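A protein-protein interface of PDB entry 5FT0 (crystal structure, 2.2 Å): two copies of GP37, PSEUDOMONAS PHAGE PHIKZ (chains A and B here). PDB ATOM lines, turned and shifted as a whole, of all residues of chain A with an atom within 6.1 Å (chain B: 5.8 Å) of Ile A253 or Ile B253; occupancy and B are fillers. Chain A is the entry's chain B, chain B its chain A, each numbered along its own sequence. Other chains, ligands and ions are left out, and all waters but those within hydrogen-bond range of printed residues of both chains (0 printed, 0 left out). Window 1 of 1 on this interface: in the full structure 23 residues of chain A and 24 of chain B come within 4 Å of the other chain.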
ATOM      1  N   ILE A 114      -7.445   5.278  28.196  1.00  0.00           N
ATOM      2  CA  ILE A 114      -7.814   6.553  28.804  1.00  0.00           C
ATOM      3  C   ILE A 114      -8.631   6.347  30.076  1.00  0.00           C
ATOM      4  O   ILE A 114      -8.626   7.207  30.963  1.00  0.00           O
ATOM      5  CB  ILE A 114      -8.570   7.453  27.804  1.00  0.00           C
ATOM      6  CG1 ILE A 114      -9.912   6.835  27.408  1.00  0.00           C
ATOM      7  CG2 ILE A 114      -7.713   7.721  26.570  1.00  0.00           C
ATOM      8  CD1 ILE A 114     -10.697   7.670  26.419  1.00  0.00           C
ATOM      9  N   GLY A 117     -13.645   0.881  32.532  1.00  0.00           N
ATOM     10  CA  GLY A 117     -15.086   0.835  32.693  1.00  0.00           C
ATOM     11  C   GLY A 117     -15.503   0.157  33.983  1.00  0.00           C
ATOM     12  O   GLY A 117     -14.818   0.266  35.001  1.00  0.00           O
ATOM     13  N   LEU A 123     -11.484   2.007  27.889  1.00  0.00           N
ATOM     14  CA  LEU A 123     -11.812   3.090  26.973  1.00  0.00           C
ATOM     15  C   LEU A 123     -10.531   3.560  26.298  1.00  0.00           C
ATOM     16  O   LEU A 123      -9.500   3.720  26.959  1.00  0.00           O
ATOM     17  CB  LEU A 123     -12.474   4.257  27.721  1.00  0.00           C
ATOM     18  CG  LEU A 123     -13.937   4.209  28.197  1.00  0.00           C
ATOM     19  CD1 LEU A 123     -14.881   4.562  27.070  1.00  0.00           C
ATOM     20  CD2 LEU A 123     -14.339   2.873  28.823  1.00  0.00           C
ATOM     21  N   ILE A 124     -10.586   3.781  24.982  1.00  0.00           N
ATOM     22  CA  ILE A 124      -9.383   4.075  24.211  1.00  0.00           C
ATOM     23  C   ILE A 124      -9.629   5.166  23.182  1.00  0.00           C
ATOM     24  O   ILE A 124     -10.733   5.319  22.651  1.00  0.00           O
ATOM     25  CB  ILE A 124      -8.836   2.827  23.488  1.00  0.00           C
ATOM     26  CG1 ILE A 124      -9.923   2.190  22.619  1.00  0.00           C
ATOM     27  CG2 ILE A 124      -8.285   1.847  24.482  1.00  0.00           C
ATOM     28  CD1 ILE A 124      -9.410   1.664  21.296  1.00  0.00           C
ATOM     29  N   LEU A 125      -8.566   5.922  22.897  1.00  0.00           N
ATOM     30  CA  LEU A 125      -8.475   6.721  21.686  1.00  0.00           C
ATOM     31  C   LEU A 125      -7.711   5.910  20.647  1.00  0.00           C
ATOM     32  O   LEU A 125      -6.510   5.659  20.841  1.00  0.00           O
ATOM     33  CB  LEU A 125      -7.763   8.041  21.954  1.00  0.00           C
ATOM     34  CG  LEU A 125      -8.522   9.202  22.590  1.00  0.00           C
ATOM     35  CD1 LEU A 125      -7.574  10.333  22.916  1.00  0.00           C
ATOM     36  CD2 LEU A 125      -9.621   9.679  21.672  1.00  0.00           C
ATOM     37  N   PRO A 126      -8.341   5.468  19.564  1.00  0.00           N
ATOM     38  CA  PRO A 126      -7.602   4.715  18.541  1.00  0.00           C
ATOM     39  C   PRO A 126      -6.503   5.565  17.917  1.00  0.00           C
ATOM     40  O   PRO A 126      -6.685   6.755  17.659  1.00  0.00           O
ATOM     41  CB  PRO A 126      -8.680   4.352  17.514  1.00  0.00           C
ATOM     42  CG  PRO A 126      -9.980   4.485  18.245  1.00  0.00           C
ATOM     43  CD  PRO A 126      -9.773   5.582  19.246  1.00  0.00           C
ATOM     44  N   PHE A 244      -7.736  16.604  30.318  1.00  0.00           N
ATOM     45  CA  PHE A 244      -8.783  15.749  29.773  1.00  0.00           C
ATOM     46  C   PHE A 244      -8.711  14.338  30.343  1.00  0.00           C
ATOM     47  O   PHE A 244      -9.738  13.763  30.723  1.00  0.00           O
ATOM     48  CB  PHE A 244      -8.683  15.721  28.248  1.00  0.00           C
ATOM     49  CG  PHE A 244      -9.655  14.787  27.593  1.00  0.00           C
ATOM     50  CD1 PHE A 244     -10.951  15.193  27.322  1.00  0.00           C
ATOM     51  CD2 PHE A 244      -9.273  13.501  27.240  1.00  0.00           C
ATOM     52  CE1 PHE A 244     -11.849  14.335  26.717  1.00  0.00           C
ATOM     53  CE2 PHE A 244     -10.167  12.637  26.634  1.00  0.00           C
ATOM     54  CZ  PHE A 244     -11.457  13.055  26.371  1.00  0.00           C
ATOM     55  N   LEU A 249     -15.154  11.542  34.695  1.00  0.00           N
ATOM     56  CA  LEU A 249     -16.302  11.149  33.888  1.00  0.00           C
ATOM     57  C   LEU A 249     -15.972  10.057  32.895  1.00  0.00           C
ATOM     58  O   LEU A 249     -16.845   9.258  32.542  1.00  0.00           O
ATOM     59  CB  LEU A 249     -16.798  12.331  33.108  1.00  0.00           C
ATOM     60  CG  LEU A 249     -17.352  13.407  33.980  1.00  0.00           C
ATOM     61  CD1 LEU A 249     -17.563  14.368  32.933  1.00  0.00           C
ATOM     62  CD2 LEU A 249     -18.641  12.941  34.597  1.00  0.00           C
ATOM     63  N   LEU A 250     -14.740  10.052  32.386  1.00  0.00           N
ATOM     64  CA  LEU A 250     -14.366   9.083  31.367  1.00  0.00           C
ATOM     65  C   LEU A 250     -14.548   7.658  31.863  1.00  0.00           C
ATOM     66  O   LEU A 250     -14.907   6.771  31.081  1.00  0.00           O
ATOM     67  CB  LEU A 250     -12.923   9.322  30.932  1.00  0.00           C
ATOM     68  CG  LEU A 250     -12.622  10.689  30.316  1.00  0.00           C
ATOM     69  CD1 LEU A 250     -11.121  10.879  30.157  1.00  0.00           C
ATOM     70  CD2 LEU A 250     -13.331  10.836  28.976  1.00  0.00           C
ATOM     71  N   SER A 251     -14.337   7.423  33.157  1.00  0.00           N
ATOM     72  CA  SER A 251     -14.468   6.090  33.730  1.00  0.00           C
ATOM     73  C   SER A 251     -15.917   5.672  33.944  1.00  0.00           C
ATOM     74  O   SER A 251     -16.157   4.564  34.435  1.00  0.00           O
ATOM     75  CB  SER A 251     -13.706   6.011  35.056  1.00  0.00           C
ATOM     76  OG  SER A 251     -14.187   6.971  35.979  1.00  0.00           O
ATOM     77  N   HIS A 252     -16.882   6.523  33.595  1.00  0.00           N
ATOM     78  CA  HIS A 252     -18.293   6.184  33.701  1.00  0.00           C
ATOM     79  C   HIS A 252     -19.001   6.210  32.356  1.00  0.00           C
ATOM     80  O   HIS A 252     -20.219   6.007  32.309  1.00  0.00           O
ATOM     81  CB  HIS A 252     -18.994   7.132  34.682  1.00  0.00           C
ATOM     82  CG  HIS A 252     -18.353   7.175  36.033  1.00  0.00           C
ATOM     83  ND1 HIS A 252     -18.383   6.109  36.905  1.00  0.00           N
ATOM     84  CD2 HIS A 252     -17.648   8.150  36.655  1.00  0.00           C
ATOM     85  CE1 HIS A 252     -17.730   6.428  38.009  1.00  0.00           C
ATOM     86  NE2 HIS A 252     -17.275   7.661  37.883  1.00  0.00           N
ATOM     87  N   ILE A 253     -18.275   6.462  31.263  1.00  0.00           N
ATOM     88  CA  ILE A 253     -18.859   6.355  29.933  1.00  0.00           C
ATOM     89  C   ILE A 253     -19.301   4.920  29.701  1.00  0.00           C
ATOM     90  O   ILE A 253     -18.527   3.974  29.892  1.00  0.00           O
ATOM     91  CB  ILE A 253     -17.851   6.816  28.868  1.00  0.00           C
ATOM     92  CG1 ILE A 253     -17.524   8.301  29.052  1.00  0.00           C
ATOM     93  CG2 ILE A 253     -18.390   6.554  27.468  1.00  0.00           C
ATOM     94  CD1 ILE A 253     -16.467   8.816  28.098  1.00  0.00           C
ATOM     95  N   ARG A 254     -20.554   4.750  29.298  1.00  0.00           N
ATOM     96  CA  ARG A 254     -21.164   3.439  29.150  1.00  0.00           C
ATOM     97  C   ARG A 254     -21.410   3.138  27.677  1.00  0.00           C
ATOM     98  O   ARG A 254     -21.732   4.031  26.888  1.00  0.00           O
ATOM     99  CB  ARG A 254     -22.480   3.367  29.936  1.00  0.00           C
ATOM    100  CG  ARG A 254     -23.358   2.165  29.627  1.00  0.00           C
ATOM    101  CD  ARG A 254     -23.114   1.057  30.636  1.00  0.00           C
ATOM    102  NE  ARG A 254     -22.951   1.586  31.987  1.00  0.00           N
ATOM    103  CZ  ARG A 254     -23.927   1.654  32.885  1.00  0.00           C
ATOM    104  NH1 ARG A 254     -25.145   1.229  32.573  1.00  0.00           N
ATOM    105  NH2 ARG A 254     -23.688   2.154  34.091  1.00  0.00           N
ATOM    106  N   THR A 255     -21.247   1.870  27.310  1.00  0.00           N
ATOM    107  CA  THR A 255     -21.525   1.403  25.960  1.00  0.00           C
ATOM    108  C   THR A 255     -22.851   0.653  25.957  1.00  0.00           C
ATOM    109  O   THR A 255     -23.021  -0.319  26.701  1.00  0.00           O
ATOM    110  CB  THR A 255     -20.406   0.500  25.450  1.00  0.00           C
ATOM    111  OG1 THR A 255     -19.142   1.050  25.834  1.00  0.00           O
ATOM    112  CG2 THR A 255     -20.461   0.394  23.936  1.00  0.00           C
ATOM    113  N   ILE B 114     -21.990  10.441  23.912  1.00  0.00           N
ATOM    114  CA  ILE B 114     -20.544  10.618  23.875  1.00  0.00           C
ATOM    115  C   ILE B 114     -19.979  10.288  22.496  1.00  0.00           C
ATOM    116  O   ILE B 114     -19.291  11.110  21.883  1.00  0.00           O
ATOM    117  CB  ILE B 114     -19.847   9.771  24.963  1.00  0.00           C
ATOM    118  CG1 ILE B 114     -20.417  10.099  26.345  1.00  0.00           C
ATOM    119  CG2 ILE B 114     -18.339   9.991  24.931  1.00  0.00           C
ATOM    120  CD1 ILE B 114     -20.337  11.559  26.708  1.00  0.00           C
ATOM    121  N   ALA B 115     -20.267   9.092  21.991  1.00  0.00           N
ATOM    122  CA  ALA B 115     -19.702   8.648  20.723  1.00  0.00           C
ATOM    123  C   ALA B 115     -20.631   7.620  20.095  1.00  0.00           C
ATOM    124  O   ALA B 115     -21.470   7.020  20.772  1.00  0.00           O
ATOM    125  CB  ALA B 115     -18.297   8.065  20.910  1.00  0.00           C
ATOM    126  N   GLY B 117     -19.428   4.916  18.455  1.00  0.00           N
ATOM    127  CA  GLY B 117     -18.838   3.595  18.610  1.00  0.00           C
ATOM    128  C   GLY B 117     -18.767   2.794  17.328  1.00  0.00           C
ATOM    129  O   GLY B 117     -18.439   3.312  16.254  1.00  0.00           O
ATOM    130  N   LEU B 123     -21.877   5.139  22.863  1.00  0.00           N
ATOM    131  CA  LEU B 123     -21.207   5.485  24.109  1.00  0.00           C
ATOM    132  C   LEU B 123     -21.961   6.651  24.734  1.00  0.00           C
ATOM    133  O   LEU B 123     -22.143   7.694  24.094  1.00  0.00           O
ATOM    134  CB  LEU B 123     -19.736   5.826  23.869  1.00  0.00           C
ATOM    135  CG  LEU B 123     -18.780   4.626  23.825  1.00  0.00           C
ATOM    136  CD1 LEU B 123     -19.095   3.668  22.679  1.00  0.00           C
ATOM    137  CD2 LEU B 123     -17.336   5.092  23.744  1.00  0.00           C
ATOM    138  N   ILE B 124     -22.424   6.465  25.967  1.00  0.00           N
ATOM    139  CA  ILE B 124     -23.322   7.408  26.626  1.00  0.00           C
ATOM    140  C   ILE B 124     -22.870   7.597  28.067  1.00  0.00           C
ATOM    141  O   ILE B 124     -22.425   6.646  28.718  1.00  0.00           O
ATOM    142  CB  ILE B 124     -24.786   6.916  26.577  1.00  0.00           C
ATOM    143  CG1 ILE B 124     -25.244   6.724  25.133  1.00  0.00           C
ATOM    144  CG2 ILE B 124     -25.717   7.883  27.297  1.00  0.00           C
ATOM    145  CD1 ILE B 124     -26.562   6.023  25.014  1.00  0.00           C
ATOM    146  N   LEU B 125     -22.980   8.831  28.563  1.00  0.00           N
ATOM    147  CA  LEU B 125     -22.738   9.117  29.968  1.00  0.00           C
ATOM    148  C   LEU B 125     -24.063   8.989  30.708  1.00  0.00           C
ATOM    149  O   LEU B 125     -24.941   9.849  30.535  1.00  0.00           O
ATOM    150  CB  LEU B 125     -22.160  10.515  30.145  1.00  0.00           C
ATOM    151  CG  LEU B 125     -21.815  10.882  31.590  1.00  0.00           C
ATOM    152  CD1 LEU B 125     -20.713   9.975  32.114  1.00  0.00           C
ATOM    153  CD2 LEU B 125     -21.411  12.341  31.694  1.00  0.00           C
ATOM    154  N   PRO B 126     -24.258   7.959  31.530  1.00  0.00           N
ATOM    155  CA  PRO B 126     -25.588   7.715  32.101  1.00  0.00           C
ATOM    156  C   PRO B 126     -25.957   8.740  33.164  1.00  0.00           C
ATOM    157  O   PRO B 126     -25.120   9.168  33.962  1.00  0.00           O
ATOM    158  CB  PRO B 126     -25.468   6.308  32.708  1.00  0.00           C
ATOM    159  CG  PRO B 126     -24.185   5.738  32.159  1.00  0.00           C
ATOM    160  CD  PRO B 126     -23.295   6.916  31.911  1.00  0.00           C
ATOM    161  N   LEU B 249     -12.294  15.134  21.142  1.00  0.00           N
ATOM    162  CA  LEU B 249     -11.777  13.793  21.402  1.00  0.00           C
ATOM    163  C   LEU B 249     -12.883  12.810  21.761  1.00  0.00           C
ATOM    164  O   LEU B 249     -12.782  11.621  21.441  1.00  0.00           O
ATOM    165  CB  LEU B 249     -10.746  13.832  22.532  1.00  0.00           C
ATOM    166  CG  LEU B 249      -9.347  14.376  22.253  1.00  0.00           C
ATOM    167  CD1 LEU B 249      -8.493  14.281  23.508  1.00  0.00           C
ATOM    168  CD2 LEU B 249      -8.699  13.620  21.102  1.00  0.00           C
ATOM    169  N   LEU B 250     -13.943  13.289  22.421  1.00  0.00           N
ATOM    170  CA  LEU B 250     -14.973  12.393  22.940  1.00  0.00           C
ATOM    171  C   LEU B 250     -15.620  11.572  21.832  1.00  0.00           C
ATOM    172  O   LEU B 250     -15.918  10.388  22.024  1.00  0.00           O
ATOM    173  CB  LEU B 250     -16.032  13.195  23.695  1.00  0.00           C
ATOM    174  CG  LEU B 250     -15.616  13.813  25.028  1.00  0.00           C
ATOM    175  CD1 LEU B 250     -16.777  14.578  25.632  1.00  0.00           C
ATOM    176  CD2 LEU B 250     -15.141  12.731  25.979  1.00  0.00           C
ATOM    177  N   SER B 251     -15.842  12.180  20.666  1.00  0.00           N
ATOM    178  CA  SER B 251     -16.486  11.466  19.568  1.00  0.00           C
ATOM    179  C   SER B 251     -15.638  10.317  19.038  1.00  0.00           C
ATOM    180  O   SER B 251     -16.187   9.380  18.448  1.00  0.00           O
ATOM    181  CB  SER B 251     -16.813  12.435  18.429  1.00  0.00           C
ATOM    182  OG  SER B 251     -15.639  13.046  17.926  1.00  0.00           O
ATOM    183  N   HIS B 252     -14.323  10.362  19.239  1.00  0.00           N
ATOM    184  CA  HIS B 252     -13.423   9.325  18.751  1.00  0.00           C
ATOM    185  C   HIS B 252     -13.185   8.218  19.768  1.00  0.00           C
ATOM    186  O   HIS B 252     -12.506   7.239  19.446  1.00  0.00           O
ATOM    187  CB  HIS B 252     -12.087   9.948  18.341  1.00  0.00           C
ATOM    188  CG  HIS B 252     -12.225  11.086  17.379  1.00  0.00           C
ATOM    189  ND1 HIS B 252     -12.609  10.909  16.068  1.00  0.00           N
ATOM    190  CD2 HIS B 252     -12.038  12.417  17.539  1.00  0.00           C
ATOM    191  CE1 HIS B 252     -12.652  12.082  15.461  1.00  0.00           C
ATOM    192  NE2 HIS B 252     -12.310  13.013  16.332  1.00  0.00           N
ATOM    193  N   ILE B 253     -13.732   8.345  20.980  1.00  0.00           N
ATOM    194  CA  ILE B 253     -13.534   7.329  22.005  1.00  0.00           C
ATOM    195  C   ILE B 253     -14.172   6.014  21.572  1.00  0.00           C
ATOM    196  O   ILE B 253     -15.251   5.993  20.967  1.00  0.00           O
ATOM    197  CB  ILE B 253     -14.113   7.817  23.345  1.00  0.00           C
ATOM    198  CG1 ILE B 253     -13.304   8.999  23.878  1.00  0.00           C
ATOM    199  CG2 ILE B 253     -14.131   6.699  24.370  1.00  0.00           C
ATOM    200  CD1 ILE B 253     -13.767   9.482  25.233  1.00  0.00           C
ATOM    201  N   ARG B 254     -13.491   4.907  21.866  1.00  0.00           N
ATOM    202  CA  ARG B 254     -14.009   3.569  21.616  1.00  0.00           C
ATOM    203  C   ARG B 254     -13.729   2.697  22.835  1.00  0.00           C
ATOM    204  O   ARG B 254     -12.895   3.027  23.683  1.00  0.00           O
ATOM    205  CB  ARG B 254     -13.388   2.941  20.359  1.00  0.00           C
ATOM    206  CG  ARG B 254     -13.620   3.723  19.074  1.00  0.00           C
ATOM    207  CD  ARG B 254     -15.091   3.741  18.683  1.00  0.00           C
ATOM    208  NE  ARG B 254     -15.305   4.445  17.421  1.00  0.00           N
ATOM    209  CZ  ARG B 254     -15.632   5.731  17.325  1.00  0.00           C
ATOM    210  NH1 ARG B 254     -15.789   6.466  18.419  1.00  0.00           N
ATOM    211  NH2 ARG B 254     -15.802   6.284  16.130  1.00  0.00           N
ATOM    212  N   THR B 255     -14.434   1.571  22.917  1.00  0.00           N
ATOM    213  CA  THR B 255     -14.363   0.689  24.073  1.00  0.00           C
ATOM    214  C   THR B 255     -13.827  -0.678  23.675  1.00  0.00           C
ATOM    215  O   THR B 255     -14.149  -1.196  22.601  1.00  0.00           O
ATOM    216  CB  THR B 255     -15.734   0.529  24.732  1.00  0.00           C
ATOM    217  OG1 THR B 255     -16.685   0.080  23.759  1.00  0.00           O
ATOM    218  CG2 THR B 255     -16.195   1.850  25.310  1.00  0.00           C
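CD1 of Leu A123 touches CG2 of Ile B253, 3.5 Å away.
Leu A123 touches Thr B255.
Ile A124 touches Ile B253 (O to CA, 3.5 Å).
Pro A126 touches His B252 (CD to O, 3.2 Å).
Phe A244 touches Leu B249.
Phe A244 touches Leu B250 (CZ to CD2, 3.7 Å).
O of His A252 touches CD of Pro B126 (3.2 Å).
Ile A253 touches Ile B114 (CD1 to CG2, 3.9 Å).
Ile A253 touches Ile B253 (CD1 to CD1, 3.99 Å).
Thr A255 touches Leu B123 (CG2 to CD1, 3.8 Å).
Leu A123 touches Ile B253, and with the chains exchanged Ile A253 touches Leu B123.
Leu A123 touches Arg B254, and with the chains exchanged Arg A254 touches Leu B123.
Ile A124 touches Arg B254, and with the chains exchanged Arg A254 touches Ile B124.
Thr A255 touches its own counterpart, Thr B255.
Of the 23 pairs that touch across the chains among the printed residues, 21 have their exchanged pair printed and touching as well.
NH1 of Arg B254 is in hydrogen-bond range of O of Ser B251, at 2.9 Å.
The backbone NH (N) of Ile B114 is in hydrogen-bond range of the backbone carbonyl oxygen (O) of Leu B123, 2.8 Å away.
The backbone carbonyl oxygen (O) of Ala B115 lies within hydrogen-bond range of the backbone NH (N) of Leu B123 (2.8 Å).
N of Ile A114 lies within hydrogen-bond range of O of Leu A123 (2.9 Å).
Of the 14 printed residues of chain A, 12 touch a printed residue of chain B.
Printed residues of chain A that touch a printed residue of chain B: Ile A114, Leu A123, Ile A124, Leu A125, Pro A126, Phe A244, Leu A249, Leu A250, His A252, Ile A253, Arg A254 and Thr A255.
Hydrophobic or aromatic side chains of chain B that line the printed part of chain A: Ile B114, Leu B123, Leu B125, Pro B126, Leu B249, Leu B250 and Ile B253.
The backbone carbonyl oxygen (O) of Arg B254 is in hydrogen-bond range of the backbone NH (N) of Ile A124 (2.8 Å).
The backbone NH (N) of Ile B124 lies within hydrogen-bond range of the backbone carbonyl oxygen (O) of Arg A254 (2.7 Å).
OG1 of Thr A255 sits close to OG1 of Thr B255 (3.4 Å).
Printed residues of chain B within 4 Å of Leu A125: Leu B249 (3.7 Å).
Printed residues of chain B within 4 Å of Pro A126: His B252 and Arg B254.
Printed residues of chain B within 4 Å of Ile A253: Ile B114 (3.9 Å), Leu B123 (3.9 Å), Ile B124 (3.7 Å) and Ile B253 (3.99 Å).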
